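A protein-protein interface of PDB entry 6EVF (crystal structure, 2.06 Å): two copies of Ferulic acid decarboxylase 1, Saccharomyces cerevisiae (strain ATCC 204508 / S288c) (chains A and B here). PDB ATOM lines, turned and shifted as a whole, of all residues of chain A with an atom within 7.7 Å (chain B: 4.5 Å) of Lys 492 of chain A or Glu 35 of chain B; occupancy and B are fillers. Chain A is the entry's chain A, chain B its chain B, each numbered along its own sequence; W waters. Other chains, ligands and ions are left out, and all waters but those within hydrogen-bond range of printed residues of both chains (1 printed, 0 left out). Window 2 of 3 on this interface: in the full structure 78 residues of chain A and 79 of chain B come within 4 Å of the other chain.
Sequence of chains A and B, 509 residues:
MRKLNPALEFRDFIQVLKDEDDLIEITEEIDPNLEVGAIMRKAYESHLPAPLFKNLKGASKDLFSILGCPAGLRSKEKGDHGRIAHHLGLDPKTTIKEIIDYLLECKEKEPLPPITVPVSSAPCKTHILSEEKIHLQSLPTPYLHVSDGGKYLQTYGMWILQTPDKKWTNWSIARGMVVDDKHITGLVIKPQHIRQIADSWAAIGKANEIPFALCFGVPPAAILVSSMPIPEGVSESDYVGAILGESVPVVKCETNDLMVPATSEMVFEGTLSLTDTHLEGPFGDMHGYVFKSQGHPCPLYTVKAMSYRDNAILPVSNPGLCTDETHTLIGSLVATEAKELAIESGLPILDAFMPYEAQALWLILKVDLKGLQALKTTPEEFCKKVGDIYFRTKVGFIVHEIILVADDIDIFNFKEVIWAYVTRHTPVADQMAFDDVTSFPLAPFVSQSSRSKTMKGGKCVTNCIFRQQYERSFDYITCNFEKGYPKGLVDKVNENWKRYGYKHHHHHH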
ATOM      1  N   PHE A 481      21.120   9.140   4.743  1.00  0.00           N
ATOM      2  CA  PHE A 481      20.367   8.091   5.336  1.00  0.00           C
ATOM      3  C   PHE A 481      19.098   8.631   5.996  1.00  0.00           C
ATOM      4  O   PHE A 481      18.004   8.244   5.610  1.00  0.00           O
ATOM      5  CB  PHE A 481      21.233   7.313   6.308  1.00  0.00           C
ATOM      6  CG  PHE A 481      20.495   6.266   7.040  1.00  0.00           C
ATOM      7  CD1 PHE A 481      19.796   5.320   6.356  1.00  0.00           C
ATOM      8  CD2 PHE A 481      20.490   6.237   8.451  1.00  0.00           C
ATOM      9  CE1 PHE A 481      19.101   4.348   7.029  1.00  0.00           C
ATOM     10  CE2 PHE A 481      19.793   5.258   9.122  1.00  0.00           C
ATOM     11  CZ  PHE A 481      19.104   4.309   8.408  1.00  0.00           C
ATOM     12  N   TYR A 485      15.279   8.806   3.085  1.00  0.00           N
ATOM     13  CA  TYR A 485      14.452   7.633   3.033  1.00  0.00           C
ATOM     14  C   TYR A 485      13.262   7.791   4.010  1.00  0.00           C
ATOM     15  O   TYR A 485      13.395   8.493   5.011  1.00  0.00           O
ATOM     16  CB  TYR A 485      15.310   6.406   3.368  1.00  0.00           C
ATOM     17  CG  TYR A 485      16.388   6.205   2.321  1.00  0.00           C
ATOM     18  CD1 TYR A 485      16.127   5.480   1.151  1.00  0.00           C
ATOM     19  CD2 TYR A 485      17.650   6.808   2.467  1.00  0.00           C
ATOM     20  CE1 TYR A 485      17.117   5.293   0.184  1.00  0.00           C
ATOM     21  CE2 TYR A 485      18.630   6.660   1.489  1.00  0.00           C
ATOM     22  CZ  TYR A 485      18.355   5.909   0.336  1.00  0.00           C
ATOM     23  OH  TYR A 485      19.323   5.807  -0.645  1.00  0.00           O
ATOM     24  N   PRO A 486      12.128   7.120   3.729  1.00  0.00           N
ATOM     25  CA  PRO A 486      10.980   7.156   4.654  1.00  0.00           C
ATOM     26  C   PRO A 486      11.334   6.753   6.100  1.00  0.00           C
ATOM     27  O   PRO A 486      12.242   5.891   6.318  1.00  0.00           O
ATOM     28  CB  PRO A 486       9.976   6.160   4.022  1.00  0.00           C
ATOM     29  CG  PRO A 486      10.497   5.800   2.686  1.00  0.00           C
ATOM     30  CD  PRO A 486      11.926   6.171   2.608  1.00  0.00           C
ATOM     31  N   LYS A 487      10.647   7.373   7.072  1.00  0.00           N
ATOM     32  CA  LYS A 487      10.853   7.064   8.473  1.00  0.00           C
ATOM     33  C   LYS A 487      10.720   5.549   8.747  1.00  0.00           C
ATOM     34  O   LYS A 487      11.507   5.003   9.496  1.00  0.00           O
ATOM     35  CB  LYS A 487       9.902   7.855   9.374  1.00  0.00           C
ATOM     36  CG  LYS A 487      10.373   7.924  10.842  1.00  0.00           C
ATOM     37  CD  LYS A 487      10.254   9.345  11.456  1.00  0.00           C
ATOM     38  CE  LYS A 487      11.237   9.616  12.605  1.00  0.00           C
ATOM     39  NZ  LYS A 487      11.121   8.648  13.740  1.00  0.00           N
ATOM     40  N   GLY A 488       9.791   4.859   8.102  1.00  0.00           N
ATOM     41  CA  GLY A 488       9.628   3.398   8.317  1.00  0.00           C
ATOM     42  C   GLY A 488      10.886   2.579   7.964  1.00  0.00           C
ATOM     43  O   GLY A 488      11.341   1.681   8.743  1.00  0.00           O
ATOM     44  N   LEU A 489      11.472   2.921   6.804  1.00  0.00           N
ATOM     45  CA  LEU A 489      12.694   2.295   6.343  1.00  0.00           C
ATOM     46  C   LEU A 489      13.897   2.642   7.208  1.00  0.00           C
ATOM     47  O   LEU A 489      14.654   1.772   7.550  1.00  0.00           O
ATOM     48  CB  LEU A 489      12.958   2.670   4.893  1.00  0.00           C
ATOM     49  CG  LEU A 489      14.134   1.955   4.270  1.00  0.00           C
ATOM     50  CD1 LEU A 489      13.965   0.464   4.407  1.00  0.00           C
ATOM     51  CD2 LEU A 489      14.230   2.376   2.818  1.00  0.00           C
ATOM     52  N   VAL A 490      14.071   3.896   7.577  1.00  0.00           N
ATOM     53  CA  VAL A 490      15.172   4.262   8.432  1.00  0.00           C
ATOM     54  C   VAL A 490      15.113   3.457   9.764  1.00  0.00           C
ATOM     55  O   VAL A 490      16.105   2.878  10.235  1.00  0.00           O
ATOM     56  CB  VAL A 490      15.151   5.766   8.699  1.00  0.00           C
ATOM     57  CG1 VAL A 490      16.072   6.158   9.855  1.00  0.00           C
ATOM     58  CG2 VAL A 490      15.498   6.551   7.412  1.00  0.00           C
ATOM     59  N   ASP A 491      13.922   3.376  10.337  1.00  0.00           N
ATOM     60  CA  ASP A 491      13.734   2.621  11.593  1.00  0.00           C
ATOM     61  C   ASP A 491      14.020   1.136  11.393  1.00  0.00           C
ATOM     62  O   ASP A 491      14.779   0.529  12.167  1.00  0.00           O
ATOM     63  CB  ASP A 491      12.312   2.867  12.177  1.00  0.00           C
ATOM     64  CG  ASP A 491      12.064   4.368  12.529  1.00  0.00           C
ATOM     65  OD1 ASP A 491      13.041   5.165  12.679  1.00  0.00           O
ATOM     66  OD2 ASP A 491      10.878   4.751  12.593  1.00  0.00           O
ATOM     67  N   LYS A 492      13.443   0.555  10.352  1.00  0.00           N
ATOM     68  CA  LYS A 492      13.695  -0.848  10.058  1.00  0.00           C
ATOM     69  C   LYS A 492      15.198  -1.147   9.908  1.00  0.00           C
ATOM     70  O   LYS A 492      15.707  -2.162  10.432  1.00  0.00           O
ATOM     71  CB  LYS A 492      12.964  -1.270   8.802  1.00  0.00           C
ATOM     72  CG  LYS A 492      13.291  -2.691   8.356  1.00  0.00           C
ATOM     73  CD  LYS A 492      12.521  -3.035   7.101  1.00  0.00           C
ATOM     74  CE  LYS A 492      12.214  -4.520   7.008  1.00  0.00           C
ATOM     75  NZ  LYS A 492      12.303  -5.008   5.603  1.00  0.00           N
ATOM     76  N   VAL A 493      15.911  -0.259   9.215  1.00  0.00           N
ATOM     77  CA  VAL A 493      17.343  -0.459   9.001  1.00  0.00           C
ATOM     78  C   VAL A 493      18.064  -0.357  10.337  1.00  0.00           C
ATOM     79  O   VAL A 493      18.876  -1.218  10.687  1.00  0.00           O
ATOM     80  CB  VAL A 493      17.898   0.541   7.960  1.00  0.00           C
ATOM     81  CG1 VAL A 493      19.425   0.672   8.039  1.00  0.00           C
ATOM     82  CG2 VAL A 493      17.441   0.116   6.556  1.00  0.00           C
ATOM     83  N   ASN A 494      17.762   0.696  11.078  1.00  0.00           N
ATOM     84  CA  ASN A 494      18.286   0.859  12.451  1.00  0.00           C
ATOM     85  C   ASN A 494      17.970  -0.317  13.405  1.00  0.00           C
ATOM     86  O   ASN A 494      18.857  -0.720  14.148  1.00  0.00           O
ATOM     87  CB  ASN A 494      17.850   2.197  13.050  1.00  0.00           C
ATOM     88  CG  ASN A 494      18.626   3.347  12.482  1.00  0.00           C
ATOM     89  OD1 ASN A 494      19.735   3.141  11.938  1.00  0.00           O
ATOM     90  ND2 ASN A 494      18.082   4.580  12.602  1.00  0.00           N
ATOM     91  N   GLU A 495      16.765  -0.881  13.339  1.00  0.00           N
ATOM     92  CA  GLU A 495      16.368  -2.041  14.199  1.00  0.00           C
ATOM     93  C   GLU A 495      17.133  -3.283  13.885  1.00  0.00           C
ATOM     94  O   GLU A 495      17.541  -3.975  14.801  1.00  0.00           O
ATOM     95  CB  GLU A 495      14.877  -2.414  14.074  1.00  0.00           C
ATOM     96  CG  GLU A 495      13.984  -1.699  15.078  1.00  0.00           C
ATOM     97  CD  GLU A 495      12.575  -1.425  14.535  1.00  0.00           C
ATOM     98  OE1 GLU A 495      12.054  -2.306  13.797  1.00  0.00           O
ATOM     99  OE2 GLU A 495      11.994  -0.336  14.844  1.00  0.00           O
ATOM    100  N   ASN A 496      17.308  -3.565  12.592  1.00  0.00           N
ATOM    101  CA  ASN A 496      17.963  -4.778  12.095  1.00  0.00           C
ATOM    102  C   ASN A 496      19.484  -4.702  11.901  1.00  0.00           C
ATOM    103  O   ASN A 496      20.113  -5.686  11.481  1.00  0.00           O
ATOM    104  CB  ASN A 496      17.325  -5.194  10.797  1.00  0.00           C
ATOM    105  CG  ASN A 496      15.851  -5.424  10.950  1.00  0.00           C
ATOM    106  OD1 ASN A 496      15.422  -6.069  11.881  1.00  0.00           O
ATOM    107  ND2 ASN A 496      15.073  -4.889  10.040  1.00  0.00           N
ATOM    108  N   TRP A 497      20.083  -3.571  12.248  1.00  0.00           N
ATOM    109  CA  TRP A 497      21.503  -3.312  11.952  1.00  0.00           C
ATOM    110  C   TRP A 497      22.380  -4.437  12.532  1.00  0.00           C
ATOM    111  O   TRP A 497      23.149  -5.085  11.804  1.00  0.00           O
ATOM    112  CB  TRP A 497      21.917  -1.927  12.502  1.00  0.00           C
ATOM    113  CG  TRP A 497      23.170  -1.355  11.884  1.00  0.00           C
ATOM    114  CD1 TRP A 497      24.328  -1.001  12.529  1.00  0.00           C
ATOM    115  CD2 TRP A 497      23.368  -1.029  10.501  1.00  0.00           C
ATOM    116  NE1 TRP A 497      25.246  -0.499  11.618  1.00  0.00           N
ATOM    117  CE2 TRP A 497      24.684  -0.524  10.370  1.00  0.00           C
ATOM    118  CE3 TRP A 497      22.565  -1.126   9.364  1.00  0.00           C
ATOM    119  CZ2 TRP A 497      25.216  -0.141   9.149  1.00  0.00           C
ATOM    120  CZ3 TRP A 497      23.091  -0.738   8.138  1.00  0.00           C
ATOM    121  CH2 TRP A 497      24.409  -0.250   8.040  1.00  0.00           C
ATOM    122  N   ARG A 499      21.465  -7.379  13.593  1.00  0.00           N
ATOM    123  CA  ARG A 499      21.090  -8.615  12.967  1.00  0.00           C
ATOM    124  C   ARG A 499      21.698  -8.800  11.582  1.00  0.00           C
ATOM    125  O   ARG A 499      22.027  -9.941  11.212  1.00  0.00           O
ATOM    126  CB  ARG A 499      19.575  -8.775  12.903  1.00  0.00           C
ATOM    127  CG  ARG A 499      19.137 -10.164  12.478  1.00  0.00           C
ATOM    128  CD  ARG A 499      17.636 -10.300  12.503  1.00  0.00           C
ATOM    129  NE  ARG A 499      17.069  -9.732  11.296  1.00  0.00           N
ATOM    130  CZ  ARG A 499      15.812  -9.327  11.165  1.00  0.00           C
ATOM    131  NH1 ARG A 499      14.952  -9.407  12.161  1.00  0.00           N
ATOM    132  NH2 ARG A 499      15.407  -8.820  10.023  1.00  0.00           N
ATOM    133  N   TYR A 500      21.860  -7.711  10.813  1.00  0.00           N
ATOM    134  CA  TYR A 500      22.571  -7.816   9.515  1.00  0.00           C
ATOM    135  C   TYR A 500      24.023  -8.369   9.711  1.00  0.00           C
ATOM    136  O   TYR A 500      24.516  -9.159   8.893  1.00  0.00           O
ATOM    137  CB  TYR A 500      22.588  -6.477   8.724  1.00  0.00           C
ATOM    138  CG  TYR A 500      21.227  -5.856   8.345  1.00  0.00           C
ATOM    139  CD1 TYR A 500      20.148  -6.626   7.974  1.00  0.00           C
ATOM    140  CD2 TYR A 500      21.058  -4.494   8.314  1.00  0.00           C
ATOM    141  CE1 TYR A 500      18.930  -6.051   7.619  1.00  0.00           C
ATOM    142  CE2 TYR A 500      19.842  -3.917   7.956  1.00  0.00           C
ATOM    143  CZ  TYR A 500      18.785  -4.709   7.599  1.00  0.00           C
ATOM    144  OH  TYR A 500      17.585  -4.156   7.240  1.00  0.00           O
ATOM    145  N   ILE B  30      16.913  -8.851   1.529  1.00  0.00           N
ATOM    146  CA  ILE B  30      16.934  -7.390   1.412  1.00  0.00           C
ATOM    147  C   ILE B  30      16.270  -7.019   0.097  1.00  0.00           C
ATOM    148  O   ILE B  30      16.490  -7.655  -0.938  1.00  0.00           O
ATOM    149  CB  ILE B  30      18.384  -6.846   1.486  1.00  0.00           C
ATOM    150  CG1 ILE B  30      19.007  -7.220   2.835  1.00  0.00           C
ATOM    151  CG2 ILE B  30      18.433  -5.329   1.269  1.00  0.00           C
ATOM    152  CD1 ILE B  30      18.388  -6.504   4.048  1.00  0.00           C
ATOM    153  N   ASP B  31      15.460  -5.971   0.142  1.00  0.00           N
ATOM    154  CA  ASP B  31      14.759  -5.488  -1.044  1.00  0.00           C
ATOM    155  C   ASP B  31      15.638  -4.519  -1.848  1.00  0.00           C
ATOM    156  O   ASP B  31      16.101  -3.527  -1.300  1.00  0.00           O
ATOM    157  CB  ASP B  31      13.505  -4.744  -0.599  1.00  0.00           C
ATOM    158  CG  ASP B  31      12.467  -4.671  -1.665  1.00  0.00           C
ATOM    159  OD1 ASP B  31      12.776  -4.718  -2.898  1.00  0.00           O
ATOM    160  OD2 ASP B  31      11.304  -4.568  -1.230  1.00  0.00           O
ATOM    161  N   PRO B  32      15.851  -4.778  -3.146  1.00  0.00           N
ATOM    162  CA  PRO B  32      16.643  -3.790  -3.885  1.00  0.00           C
ATOM    163  C   PRO B  32      15.899  -2.443  -4.010  1.00  0.00           C
ATOM    164  O   PRO B  32      16.538  -1.444  -4.202  1.00  0.00           O
ATOM    165  CB  PRO B  32      16.865  -4.477  -5.253  1.00  0.00           C
ATOM    166  CG  PRO B  32      15.787  -5.488  -5.368  1.00  0.00           C
ATOM    167  CD  PRO B  32      15.534  -5.956  -3.984  1.00  0.00           C
ATOM    168  N   ASN B  33      14.565  -2.451  -3.871  1.00  0.00           N
ATOM    169  CA  ASN B  33      13.735  -1.239  -3.740  1.00  0.00           C
ATOM    170  C   ASN B  33      14.006  -0.460  -2.445  1.00  0.00           C
ATOM    171  O   ASN B  33      13.519  -0.825  -1.401  1.00  0.00           O
ATOM    172  CB  ASN B  33      12.237  -1.592  -3.875  1.00  0.00           C
ATOM    173  CG  ASN B  33      11.352  -0.374  -3.904  1.00  0.00           C
ATOM    174  OD1 ASN B  33      11.775   0.678  -4.312  1.00  0.00           O
ATOM    175  ND2 ASN B  33      10.115  -0.523  -3.496  1.00  0.00           N
ATOM    176  N   LEU B  34      14.814   0.606  -2.544  1.00  0.00           N
ATOM    177  CA  LEU B  34      15.180   1.509  -1.444  1.00  0.00           C
ATOM    178  C   LEU B  34      16.103   0.917  -0.373  1.00  0.00           C
ATOM    179  O   LEU B  34      17.012   1.590   0.048  1.00  0.00           O
ATOM    180  CB  LEU B  34      13.957   2.215  -0.802  1.00  0.00           C
ATOM    181  CG  LEU B  34      13.074   3.082  -1.731  1.00  0.00           C
ATOM    182  CD1 LEU B  34      11.950   3.794  -0.976  1.00  0.00           C
ATOM    183  CD2 LEU B  34      13.929   4.137  -2.487  1.00  0.00           C
ATOM    184  N   GLU B  35      15.913  -0.343   0.028  1.00  0.00           N
ATOM    185  CA  GLU B  35      16.521  -0.885   1.245  1.00  0.00           C
ATOM    186  C   GLU B  35      18.024  -1.060   1.098  1.00  0.00           C
ATOM    187  O   GLU B  35      18.758  -0.773   1.997  1.00  0.00           O
ATOM    188  CB  GLU B  35      15.824  -2.192   1.579  1.00  0.00           C
ATOM    189  CG  GLU B  35      16.065  -2.678   2.992  1.00  0.00           C
ATOM    190  CD  GLU B  35      15.175  -3.864   3.404  1.00  0.00           C
ATOM    191  OE1 GLU B  35      14.672  -4.597   2.522  1.00  0.00           O
ATOM    192  OE2 GLU B  35      14.996  -4.039   4.632  1.00  0.00           O
ATOM    193  N   VAL B  36      18.474  -1.524  -0.056  1.00  0.00           N
ATOM    194  CA  VAL B  36      19.896  -1.588  -0.370  1.00  0.00           C
ATOM    195  C   VAL B  36      20.534  -0.194  -0.272  1.00  0.00           C
ATOM    196  O   VAL B  36      21.550  -0.009   0.408  1.00  0.00           O
ATOM    197  CB  VAL B  36      20.081  -2.118  -1.805  1.00  0.00           C
ATOM    198  CG1 VAL B  36      21.466  -1.898  -2.328  1.00  0.00           C
ATOM    199  CG2 VAL B  36      19.764  -3.586  -1.821  1.00  0.00           C
ATOM    200  N   GLY B  37      19.917   0.787  -0.907  1.00  0.00           N
ATOM    201  CA  GLY B  37      20.474   2.099  -0.942  1.00  0.00           C
ATOM    202  C   GLY B  37      20.518   2.753   0.432  1.00  0.00           C
ATOM    203  O   GLY B  37      21.436   3.485   0.737  1.00  0.00           O
ATOM    204  N   ALA B  38      19.515   2.482   1.258  1.00  0.00           N
ATOM    205  CA  ALA B  38      19.424   3.065   2.616  1.00  0.00           C
ATOM    206  C   ALA B  38      20.492   2.463   3.547  1.00  0.00           C
ATOM    207  O   ALA B  38      21.149   3.189   4.303  1.00  0.00           O
ATOM    208  CB  ALA B  38      18.020   2.843   3.176  1.00  0.00           C
ATOM    209  N   ILE B  39      20.664   1.140   3.467  1.00  0.00           N
ATOM    210  CA  ILE B  39      21.737   0.422   4.196  1.00  0.00           C
ATOM    211  C   ILE B  39      23.116   0.972   3.805  1.00  0.00           C
ATOM    212  O   ILE B  39      23.920   1.294   4.686  1.00  0.00           O
ATOM    213  CB  ILE B  39      21.625  -1.081   3.934  1.00  0.00           C
ATOM    214  CG1 ILE B  39      20.506  -1.651   4.825  1.00  0.00           C
ATOM    215  CG2 ILE B  39      22.940  -1.782   4.195  1.00  0.00           C
ATOM    216  CD1 ILE B  39      19.964  -2.953   4.358  1.00  0.00           C
HETATM  217  O   HOH W   1      13.896  -7.072   3.474  1.00  0.00           O
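O of Gly 37 of chain B sits at hydrogen-bond distance from OH of Tyr 485 of chain A (3.4 Å).
The side-chain amino group (NZ) of Lys 492 of chain A is in salt-bridge range of the side-chain carboxylate (OE2) of Glu 35 of chain B, at 3.0 Å.
The backbone carbonyl oxygen (O) of Lys 492 of chain A is in hydrogen-bond range of the side-chain amide nitrogen (ND2) of Asn 496 of chain A (2.8 Å).
OE1 of Glu 35 of chain B lies within hydrogen-bond range of N of Asp 31 of chain B.
Phe 481 of chain A touches Ala 38 of chain B (CD1 to O, 3.3 Å).
Leu 34 of chain B touches Tyr 485 of chain A (O to CE1, 3.7 Å).
N of Ala 38 of chain B touches CZ of Tyr 485 of chain A (3.7 Å).
Leu 489 of chain A touches Leu 34 of chain B (CD2 to CB, 3.6 Å).
CB of Ala 38 of chain B touches CD2 of Leu 489 of chain A (3.8 Å).
CG2 of Val 493 of chain A touches CG1 of Ile 39 of chain B (3.9 Å).
Ile 39 of chain B touches Trp 497 of chain A.
Tyr 500 of chain A touches Ile 30 of chain B (CE1 to CD1, 3.6 Å).
OH of Tyr 500 of chain A touches OE2 of Glu 35 of chain B (3.7 Å).
CE2 of Tyr 500 of chain A touches CD1 of Ile 39 of chain B (3.7 Å).
Val 490 of chain A touches none of the printed residues of chain B.
Of chain B, only Glu 35 (3.0 Å) comes within 4 Å of Lys 492 of chain A.
Of the printed residues of chain B, Val 493 of chain A touches Ile 39 (3.9 Å).
Of the printed residues of chain B, Tyr 500 of chain A touches Ile 30 (3.6 Å), Glu 35 (3.7 Å) and Ile 39 (3.7 Å).
Of the printed residues of chain A, Leu 34 of chain B touches Tyr 485 (3.7 Å) and Leu 489 (3.6 Å).
Glu 35 of chain B touches two residues of chain A.
The nearest printed residue of chain B that does not touch Lys 492 of chain A is Asp 31 of chain B (6.3 Å).
The nearest printed residue of chain A that does not touch Leu 34 of chain B is Pro 486 of chain A (4.3 Å).
Of the 10 printed residues of chain B, 6 touch a printed residue of chain A.
Of the 16 printed residues of chain A, 7 touch a printed residue of chain B.
Among the printed residues, Asp or Glu carboxylates within 4 Å of a Lys or Arg side-chain nitrogen of the other chain: Lys 492 of chain A with Glu 35 of chain B.
No position is printed for both chains.
Water W1 lies within hydrogen-bond range of OE1 of Glu 35 of chain B (2.8 Å) and NZ of Lys 492 of chain A (3.4 Å).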
